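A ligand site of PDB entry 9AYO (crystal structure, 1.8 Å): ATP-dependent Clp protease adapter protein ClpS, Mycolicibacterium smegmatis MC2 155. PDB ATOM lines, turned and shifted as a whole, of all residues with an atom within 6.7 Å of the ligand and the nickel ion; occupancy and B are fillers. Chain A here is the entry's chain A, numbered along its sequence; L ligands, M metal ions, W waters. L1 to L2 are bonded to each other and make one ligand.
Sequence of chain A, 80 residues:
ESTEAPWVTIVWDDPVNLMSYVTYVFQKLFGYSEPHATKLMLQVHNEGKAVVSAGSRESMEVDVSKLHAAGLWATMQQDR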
ATOM      1  N   VAL A  11      -0.272  18.026  10.277  1.00  0.00           N
ATOM      2  CA  VAL A  11      -1.277  16.980  10.381  1.00  0.00           C
ATOM      3  C   VAL A  11      -0.837  16.007  11.470  1.00  0.00           C
ATOM      4  O   VAL A  11       0.339  15.637  11.542  1.00  0.00           O
ATOM      5  CB  VAL A  11      -1.495  16.268   9.044  1.00  0.00           C
ATOM      6  CG1 VAL A  11      -2.384  15.051   9.212  1.00  0.00           C
ATOM      7  CG2 VAL A  11      -2.110  17.234   8.036  1.00  0.00           C
ATOM      8  N   TRP A  12      -1.781  15.608  12.316  1.00  0.00           N
ATOM      9  CA  TRP A  12      -1.516  14.771  13.465  1.00  0.00           C
ATOM     10  C   TRP A  12      -2.124  13.391  13.246  1.00  0.00           C
ATOM     11  O   TRP A  12      -3.200  13.263  12.666  1.00  0.00           O
ATOM     12  CB  TRP A  12      -2.127  15.402  14.727  1.00  0.00           C
ATOM     13  CG  TRP A  12      -1.560  16.746  15.047  1.00  0.00           C
ATOM     14  CD1 TRP A  12      -1.958  17.946  14.536  1.00  0.00           C
ATOM     15  CD2 TRP A  12      -0.498  17.032  15.960  1.00  0.00           C
ATOM     16  NE1 TRP A  12      -1.203  18.964  15.076  1.00  0.00           N
ATOM     17  CE2 TRP A  12      -0.303  18.431  15.945  1.00  0.00           C
ATOM     18  CE3 TRP A  12       0.304  16.243  16.786  1.00  0.00           C
ATOM     19  CZ2 TRP A  12       0.667  19.050  16.728  1.00  0.00           C
ATOM     20  CZ3 TRP A  12       1.266  16.862  17.563  1.00  0.00           C
ATOM     21  CH2 TRP A  12       1.442  18.256  17.524  1.00  0.00           C
ATOM     22  N   ASP A  13      -1.408  12.366  13.702  1.00  0.00           N
ATOM     23  CA  ASP A  13      -1.891  11.000  13.551  1.00  0.00           C
ATOM     24  C   ASP A  13      -3.178  10.813  14.338  1.00  0.00           C
ATOM     25  O   ASP A  13      -3.339  11.352  15.428  1.00  0.00           O
ATOM     26  CB  ASP A  13      -0.822  10.026  14.042  1.00  0.00           C
ATOM     27  CG  ASP A  13      -1.191   8.585  13.767  1.00  0.00           C
ATOM     28  OD1 ASP A  13      -1.661   8.307  12.637  1.00  0.00           O
ATOM     29  OD2 ASP A  13      -0.999   7.729  14.647  1.00  0.00           O
ATOM     30  N   ASP A  14      -4.110  10.038  13.773  1.00  0.00           N
ATOM     31  CA  ASP A  14      -5.360   9.710  14.431  1.00  0.00           C
ATOM     32  C   ASP A  14      -5.687   8.253  14.134  1.00  0.00           C
ATOM     33  O   ASP A  14      -5.263   7.706  13.109  1.00  0.00           O
ATOM     34  CB  ASP A  14      -6.502  10.610  13.948  1.00  0.00           C
ATOM     35  CG  ASP A  14      -7.063  10.199  12.611  1.00  0.00           C
ATOM     36  OD1 ASP A  14      -7.917   9.290  12.578  1.00  0.00           O
ATOM     37  OD2 ASP A  14      -6.671  10.794  11.583  1.00  0.00           O
ATOM     38  N   PRO A  15      -6.439   7.596  15.033  1.00  0.00           N
ATOM     39  CA  PRO A  15      -6.625   6.142  14.914  1.00  0.00           C
ATOM     40  C   PRO A  15      -7.739   5.711  13.974  1.00  0.00           C
ATOM     41  O   PRO A  15      -7.921   4.506  13.773  1.00  0.00           O
ATOM     42  CB  PRO A  15      -6.942   5.726  16.358  1.00  0.00           C
ATOM     43  CG  PRO A  15      -7.673   6.916  16.916  1.00  0.00           C
ATOM     44  CD  PRO A  15      -7.045   8.142  16.266  1.00  0.00           C
ATOM     45  N   VAL A  16      -8.509   6.635  13.400  1.00  0.00           N
ATOM     46  CA  VAL A  16      -9.680   6.303  12.610  1.00  0.00           C
ATOM     47  C   VAL A  16      -9.401   6.360  11.118  1.00  0.00           C
ATOM     48  O   VAL A  16      -9.691   5.413  10.387  1.00  0.00           O
ATOM     49  CB  VAL A  16     -10.871   7.209  13.004  1.00  0.00           C
ATOM     50  CG1 VAL A  16     -12.100   6.903  12.144  1.00  0.00           C
ATOM     51  CG2 VAL A  16     -11.196   7.055  14.481  1.00  0.00           C
ATOM     52  N   ASN A  17      -8.839   7.465  10.643  1.00  0.00           N
ATOM     53  CA  ASN A  17      -8.664   7.662   9.202  1.00  0.00           C
ATOM     54  C   ASN A  17      -7.742   6.597   8.617  1.00  0.00           C
ATOM     55  O   ASN A  17      -6.735   6.219   9.227  1.00  0.00           O
ATOM     56  CB  ASN A  17      -8.081   9.052   8.940  1.00  0.00           C
ATOM     57  CG  ASN A  17      -9.131  10.136   8.949  1.00  0.00           C
ATOM     58  OD1 ASN A  17     -10.145  10.048   8.255  1.00  0.00           O
ATOM     59  ND2 ASN A  17      -8.904  11.170   9.755  1.00  0.00           N
ATOM     60  N   LEU A  18      -8.094   6.137   7.431  1.00  0.00           N
ATOM     61  CA  LEU A  18      -7.292   5.130   6.745  1.00  0.00           C
ATOM     62  C   LEU A  18      -6.018   5.746   6.180  1.00  0.00           C
ATOM     63  O   LEU A  18      -6.031   6.875   5.686  1.00  0.00           O
ATOM     64  CB  LEU A  18      -8.095   4.523   5.593  1.00  0.00           C
ATOM     65  CG  LEU A  18      -9.276   3.617   5.942  1.00  0.00           C
ATOM     66  CD1 LEU A  18     -10.125   3.375   4.702  1.00  0.00           C
ATOM     67  CD2 LEU A  18      -8.772   2.310   6.518  1.00  0.00           C
ATOM     68  N   MET A  19      -4.928   4.984   6.248  1.00  0.00           N
ATOM     69  CA  MET A  19      -3.690   5.426   5.614  1.00  0.00           C
ATOM     70  C   MET A  19      -3.931   5.787   4.157  1.00  0.00           C
ATOM     71  O   MET A  19      -3.430   6.811   3.672  1.00  0.00           O
ATOM     72  CB  MET A  19      -2.632   4.333   5.710  1.00  0.00           C
ATOM     73  CG  MET A  19      -2.222   3.971   7.126  1.00  0.00           C
ATOM     74  SD  MET A  19      -1.011   2.631   7.147  1.00  0.00           S
ATOM     75  CE  MET A  19       0.450   3.492   6.558  1.00  0.00           C
ATOM     76  N   SER A  20      -4.674   4.949   3.436  1.00  0.00           N
ATOM     77  CA  SER A  20      -4.934   5.218   2.028  1.00  0.00           C
ATOM     78  C   SER A  20      -5.704   6.516   1.853  1.00  0.00           C
ATOM     79  O   SER A  20      -5.469   7.274   0.899  1.00  0.00           O
ATOM     80  CB  SER A  20      -5.722   4.054   1.421  1.00  0.00           C
ATOM     81  OG  SER A  20      -6.974   3.903   2.065  1.00  0.00           O
ATOM     82  N   TYR A  21      -6.642   6.803   2.770  1.00  0.00           N
ATOM     83  CA  TYR A  21      -7.407   8.036   2.681  1.00  0.00           C
ATOM     84  C   TYR A  21      -6.515   9.253   2.842  1.00  0.00           C
ATOM     85  O   TYR A  21      -6.635  10.223   2.093  1.00  0.00           O
ATOM     86  CB  TYR A  21      -8.504   8.031   3.748  1.00  0.00           C
ATOM     87  CG  TYR A  21      -9.356   9.288   3.743  1.00  0.00           C
ATOM     88  CD1 TYR A  21     -10.168   9.601   2.671  1.00  0.00           C
ATOM     89  CD2 TYR A  21      -9.343  10.158   4.834  1.00  0.00           C
ATOM     90  CE1 TYR A  21     -10.949  10.734   2.660  1.00  0.00           C
ATOM     91  CE2 TYR A  21     -10.115  11.305   4.830  1.00  0.00           C
ATOM     92  CZ  TYR A  21     -10.920  11.589   3.746  1.00  0.00           C
ATOM     93  OH  TYR A  21     -11.693  12.722   3.741  1.00  0.00           O
ATOM     94  N   VAL A  22      -5.595   9.205   3.813  1.00  0.00           N
ATOM     95  CA  VAL A  22      -4.743  10.365   4.070  1.00  0.00           C
ATOM     96  C   VAL A  22      -3.874  10.662   2.850  1.00  0.00           C
ATOM     97  O   VAL A  22      -3.736  11.831   2.442  1.00  0.00           O
ATOM     98  CB  VAL A  22      -3.891  10.132   5.329  1.00  0.00           C
ATOM     99  CG1 VAL A  22      -2.928  11.279   5.555  1.00  0.00           C
ATOM    100  CG2 VAL A  22      -4.807   9.944   6.538  1.00  0.00           C
ATOM    101  N   PHE A  26      -4.033  14.247   0.714  1.00  0.00           N
ATOM    102  CA  PHE A  26      -2.889  15.112   0.444  1.00  0.00           C
ATOM    103  C   PHE A  26      -2.757  15.397  -1.049  1.00  0.00           C
ATOM    104  O   PHE A  26      -2.380  16.518  -1.444  1.00  0.00           O
ATOM    105  CB  PHE A  26      -1.598  14.494   0.972  1.00  0.00           C
ATOM    106  CG  PHE A  26      -1.505  14.451   2.488  1.00  0.00           C
ATOM    107  CD1 PHE A  26      -2.369  15.183   3.282  1.00  0.00           C
ATOM    108  CD2 PHE A  26      -0.527  13.678   3.100  1.00  0.00           C
ATOM    109  CE1 PHE A  26      -2.272  15.143   4.659  1.00  0.00           C
ATOM    110  CE2 PHE A  26      -0.430  13.638   4.478  1.00  0.00           C
ATOM    111  CZ  PHE A  26      -1.299  14.364   5.260  1.00  0.00           C
ATOM    112  N   LEU A  40       4.521  11.918   3.175  1.00  0.00           N
ATOM    113  CA  LEU A  40       3.965  12.719   4.264  1.00  0.00           C
ATOM    114  C   LEU A  40       3.037  11.880   5.148  1.00  0.00           C
ATOM    115  O   LEU A  40       3.105  11.973   6.377  1.00  0.00           O
ATOM    116  CB  LEU A  40       3.222  13.918   3.695  1.00  0.00           C
ATOM    117  CG  LEU A  40       4.083  14.969   3.003  1.00  0.00           C
ATOM    118  CD1 LEU A  40       3.191  15.987   2.299  1.00  0.00           C
ATOM    119  CD2 LEU A  40       5.014  15.664   3.993  1.00  0.00           C
ATOM    120  N   MET A  41       2.177  11.061   4.533  1.00  0.00           N
ATOM    121  CA  MET A  41       1.296  10.214   5.321  1.00  0.00           C
ATOM    122  C   MET A  41       2.089   9.310   6.249  1.00  0.00           C
ATOM    123  O   MET A  41       1.727   9.129   7.424  1.00  0.00           O
ATOM    124  CB  MET A  41       0.397   9.389   4.393  1.00  0.00           C
ATOM    125  CG  MET A  41      -0.557   8.441   5.119  1.00  0.00           C
ATOM    126  SD  MET A  41       0.190   6.869   5.582  1.00  0.00           S
ATOM    127  CE  MET A  41       0.474   6.128   3.978  1.00  0.00           C
ATOM    128  N   LEU A  42       3.173   8.717   5.742  1.00  0.00           N
ATOM    129  CA  LEU A  42       3.969   7.828   6.584  1.00  0.00           C
ATOM    130  C   LEU A  42       4.721   8.588   7.668  1.00  0.00           C
ATOM    131  O   LEU A  42       4.903   8.074   8.774  1.00  0.00           O
ATOM    132  CB  LEU A  42       4.934   7.015   5.717  1.00  0.00           C
ATOM    133  CG  LEU A  42       4.282   5.984   4.793  1.00  0.00           C
ATOM    134  CD1 LEU A  42       5.313   5.374   3.856  1.00  0.00           C
ATOM    135  CD2 LEU A  42       3.584   4.901   5.599  1.00  0.00           C
ATOM    136  N   VAL A  44       3.613  11.237   9.223  1.00  0.00           N
ATOM    137  CA  VAL A  44       2.596  11.419  10.268  1.00  0.00           C
ATOM    138  C   VAL A  44       2.427  10.137  11.071  1.00  0.00           C
ATOM    139  O   VAL A  44       2.446  10.154  12.308  1.00  0.00           O
ATOM    140  CB  VAL A  44       1.262  11.879   9.649  1.00  0.00           C
ATOM    141  CG1 VAL A  44       0.191  11.993  10.725  1.00  0.00           C
ATOM    142  CG2 VAL A  44       1.430  13.188   8.916  1.00  0.00           C
ATOM    143  N   HIS A  45       2.249   9.014  10.374  1.00  0.00           N
ATOM    144  CA  HIS A  45       1.931   7.770  11.063  1.00  0.00           C
ATOM    145  C   HIS A  45       3.097   7.308  11.936  1.00  0.00           C
ATOM    146  O   HIS A  45       2.877   6.760  13.023  1.00  0.00           O
ATOM    147  CB  HIS A  45       1.573   6.698  10.044  1.00  0.00           C
ATOM    148  CG  HIS A  45       0.664   5.632  10.567  1.00  0.00           C
ATOM    149  ND1 HIS A  45       0.663   4.345  10.087  1.00  0.00           N
ATOM    150  CD2 HIS A  45      -0.281   5.663  11.536  1.00  0.00           C
ATOM    151  CE1 HIS A  45      -0.239   3.630  10.732  1.00  0.00           C
ATOM    152  NE2 HIS A  45      -0.830   4.409  11.617  1.00  0.00           N
ATOM    153  N   LEU A  72      -9.354  15.306   8.851  1.00  0.00           N
ATOM    154  CA  LEU A  72      -8.016  15.082   9.370  1.00  0.00           C
ATOM    155  C   LEU A  72      -7.707  16.070  10.478  1.00  0.00           C
ATOM    156  O   LEU A  72      -8.202  17.201  10.489  1.00  0.00           O
ATOM    157  CB  LEU A  72      -6.975  15.218   8.257  1.00  0.00           C
ATOM    158  CG  LEU A  72      -6.683  13.958   7.440  1.00  0.00           C
ATOM    159  CD1 LEU A  72      -7.934  13.429   6.771  1.00  0.00           C
ATOM    160  CD2 LEU A  72      -5.592  14.239   6.406  1.00  0.00           C
ATOM    161  N   TRP A  73      -6.869  15.638  11.422  1.00  0.00           N
ATOM    162  CA  TRP A  73      -6.461  16.493  12.537  1.00  0.00           C
ATOM    163  C   TRP A  73      -5.345  17.399  12.059  1.00  0.00           C
ATOM    164  O   TRP A  73      -4.194  16.958  11.892  1.00  0.00           O
ATOM    165  CB  TRP A  73      -5.983  15.644  13.704  1.00  0.00           C
ATOM    166  CG  TRP A  73      -7.036  14.774  14.319  1.00  0.00           C
ATOM    167  CD1 TRP A  73      -8.346  14.710  13.969  1.00  0.00           C
ATOM    168  CD2 TRP A  73      -6.854  13.858  15.406  1.00  0.00           C
ATOM    169  NE1 TRP A  73      -9.005  13.802  14.774  1.00  0.00           N
ATOM    170  CE2 TRP A  73      -8.105  13.268  15.660  1.00  0.00           C
ATOM    171  CE3 TRP A  73      -5.758  13.479  16.180  1.00  0.00           C
ATOM    172  CZ2 TRP A  73      -8.295  12.309  16.653  1.00  0.00           C
ATOM    173  CZ3 TRP A  73      -5.944  12.527  17.167  1.00  0.00           C
ATOM    174  CH2 TRP A  73      -7.201  11.952  17.399  1.00  0.00           C
HETATM  175  N1  LIG L   1      -3.345   6.021  12.165  1.00  0.00           N
HETATM  176  C1  LIG L   1      -4.105   5.711  10.933  1.00  0.00           C
HETATM  177  C2  LIG L   1      -4.392   4.219  10.862  1.00  0.00           C
HETATM  178  O1  LIG L   1      -3.648   3.396  11.397  1.00  0.00           O
HETATM  179  C3  LIG L   1      -3.321   6.160   9.707  1.00  0.00           C
HETATM  180  C4  LIG L   1      -3.090   7.651   9.620  1.00  0.00           C
HETATM  181  C5  LIG L   1      -4.000   8.539  10.173  1.00  0.00           C
HETATM  182  C6  LIG L   1      -1.963   8.156   8.990  1.00  0.00           C
HETATM  183  C7  LIG L   1      -3.789   9.896  10.101  1.00  0.00           C
HETATM  184  C8  LIG L   1      -1.744   9.512   8.924  1.00  0.00           C
HETATM  185  C9  LIG L   1      -2.655  10.386   9.477  1.00  0.00           C
HETATM  186  N1  LG2 L   2      -5.478   3.866  10.173  1.00  0.00           N
HETATM  187  C1  LG2 L   2      -5.909   2.489  10.053  1.00  0.00           C
HETATM  188  C2  LG2 L   2      -5.538   1.901   8.696  1.00  0.00           C
HETATM  189  O1  LG2 L   2      -5.532   0.687   8.513  1.00  0.00           O
HETATM  190  C3  LG2 L   2      -7.410   2.382  10.267  1.00  0.00           C
HETATM  191  O2  LG2 L   2      -5.235   2.634   7.749  1.00  0.00           O
HETATM  192 NI    NI M   1      -2.319   4.169  12.748  1.00  0.00          NI
HETATM  193 MG    MG M   2      -5.469  13.153  11.139  1.00  0.00          MG
HETATM  194  O   HOH W   1      -3.681   3.897  14.074  1.00  0.00           O
HETATM  195  O   HOH W   2      -1.411   2.253  13.315  1.00  0.00           O
HETATM  196  O   HOH W   3      -6.194  -0.680   6.375  1.00  0.00           O
HETATM  197  O   HOH W   4      -1.177   5.025  14.321  1.00  0.00           O
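Of the 20 residues printed, 1 comes within 4 Å of the nickel ion.
SD of Met 19 lies close to ND1 of His 45, 3.8 Å away. The side-chain carboxylate of Asp 14 sits at hydrogen-bond distance from the backbone NH of Asn 17 (2.8 Å). The side-chain carboxylate (OD1) of Asp 14 sits at hydrogen-bond distance from the backbone NH (N) of Val 16, at 2.8 Å.
O of Asn 17 sits at hydrogen-bond distance from N1 of LG2 L2. The backbone carbonyl oxygen of Asp 14 lies close to a nitrogen (N1) of LIG L1 (2.7 Å). N of Met 19 is in hydrogen-bond range of O2 of LG2 L2 (2.8 Å). N1 of LIG L1 sits close to OD1 of Asp 13 (2.9 Å).
Val 16 touches the ligand. CA of Leu 18 touches O2 of LG2 L2, at 3.4 Å. Val 22 touches the ligand. Met 41 touches the ligand. CG1 of Val 44 touches C9 of LIG L1 (3.5 Å). Hydrophobic or aromatic side chains within 4 Å of the ligand: Leu 18, Met 19, Val 22, Val 44 and His 45. Ten residues have an atom within 4 Å of the ligand: Asp 13, Asp 14, Val 16, Asn 17, Leu 18, Met 19, Val 22, Met 41, Val 44 and His 45. The nearest printed residue that does not touch the ligand is Pro 15 (4.1 Å).
The nickel ion is bound by a ring nitrogen (NE2) of His 45. Water W1 binds the nickel ion (1.9 Å). An oxygen (O1) of LIG L1 is bound to the nickel ion (2.0 Å). The nickel ion is bound by water W4 (2.1 Å). Water W2 is bound to the nickel ion (2.2 Å). The nickel ion is bound by N1 of LIG L1 (2.2 Å). The nickel ion has six donor atoms within binding distance.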
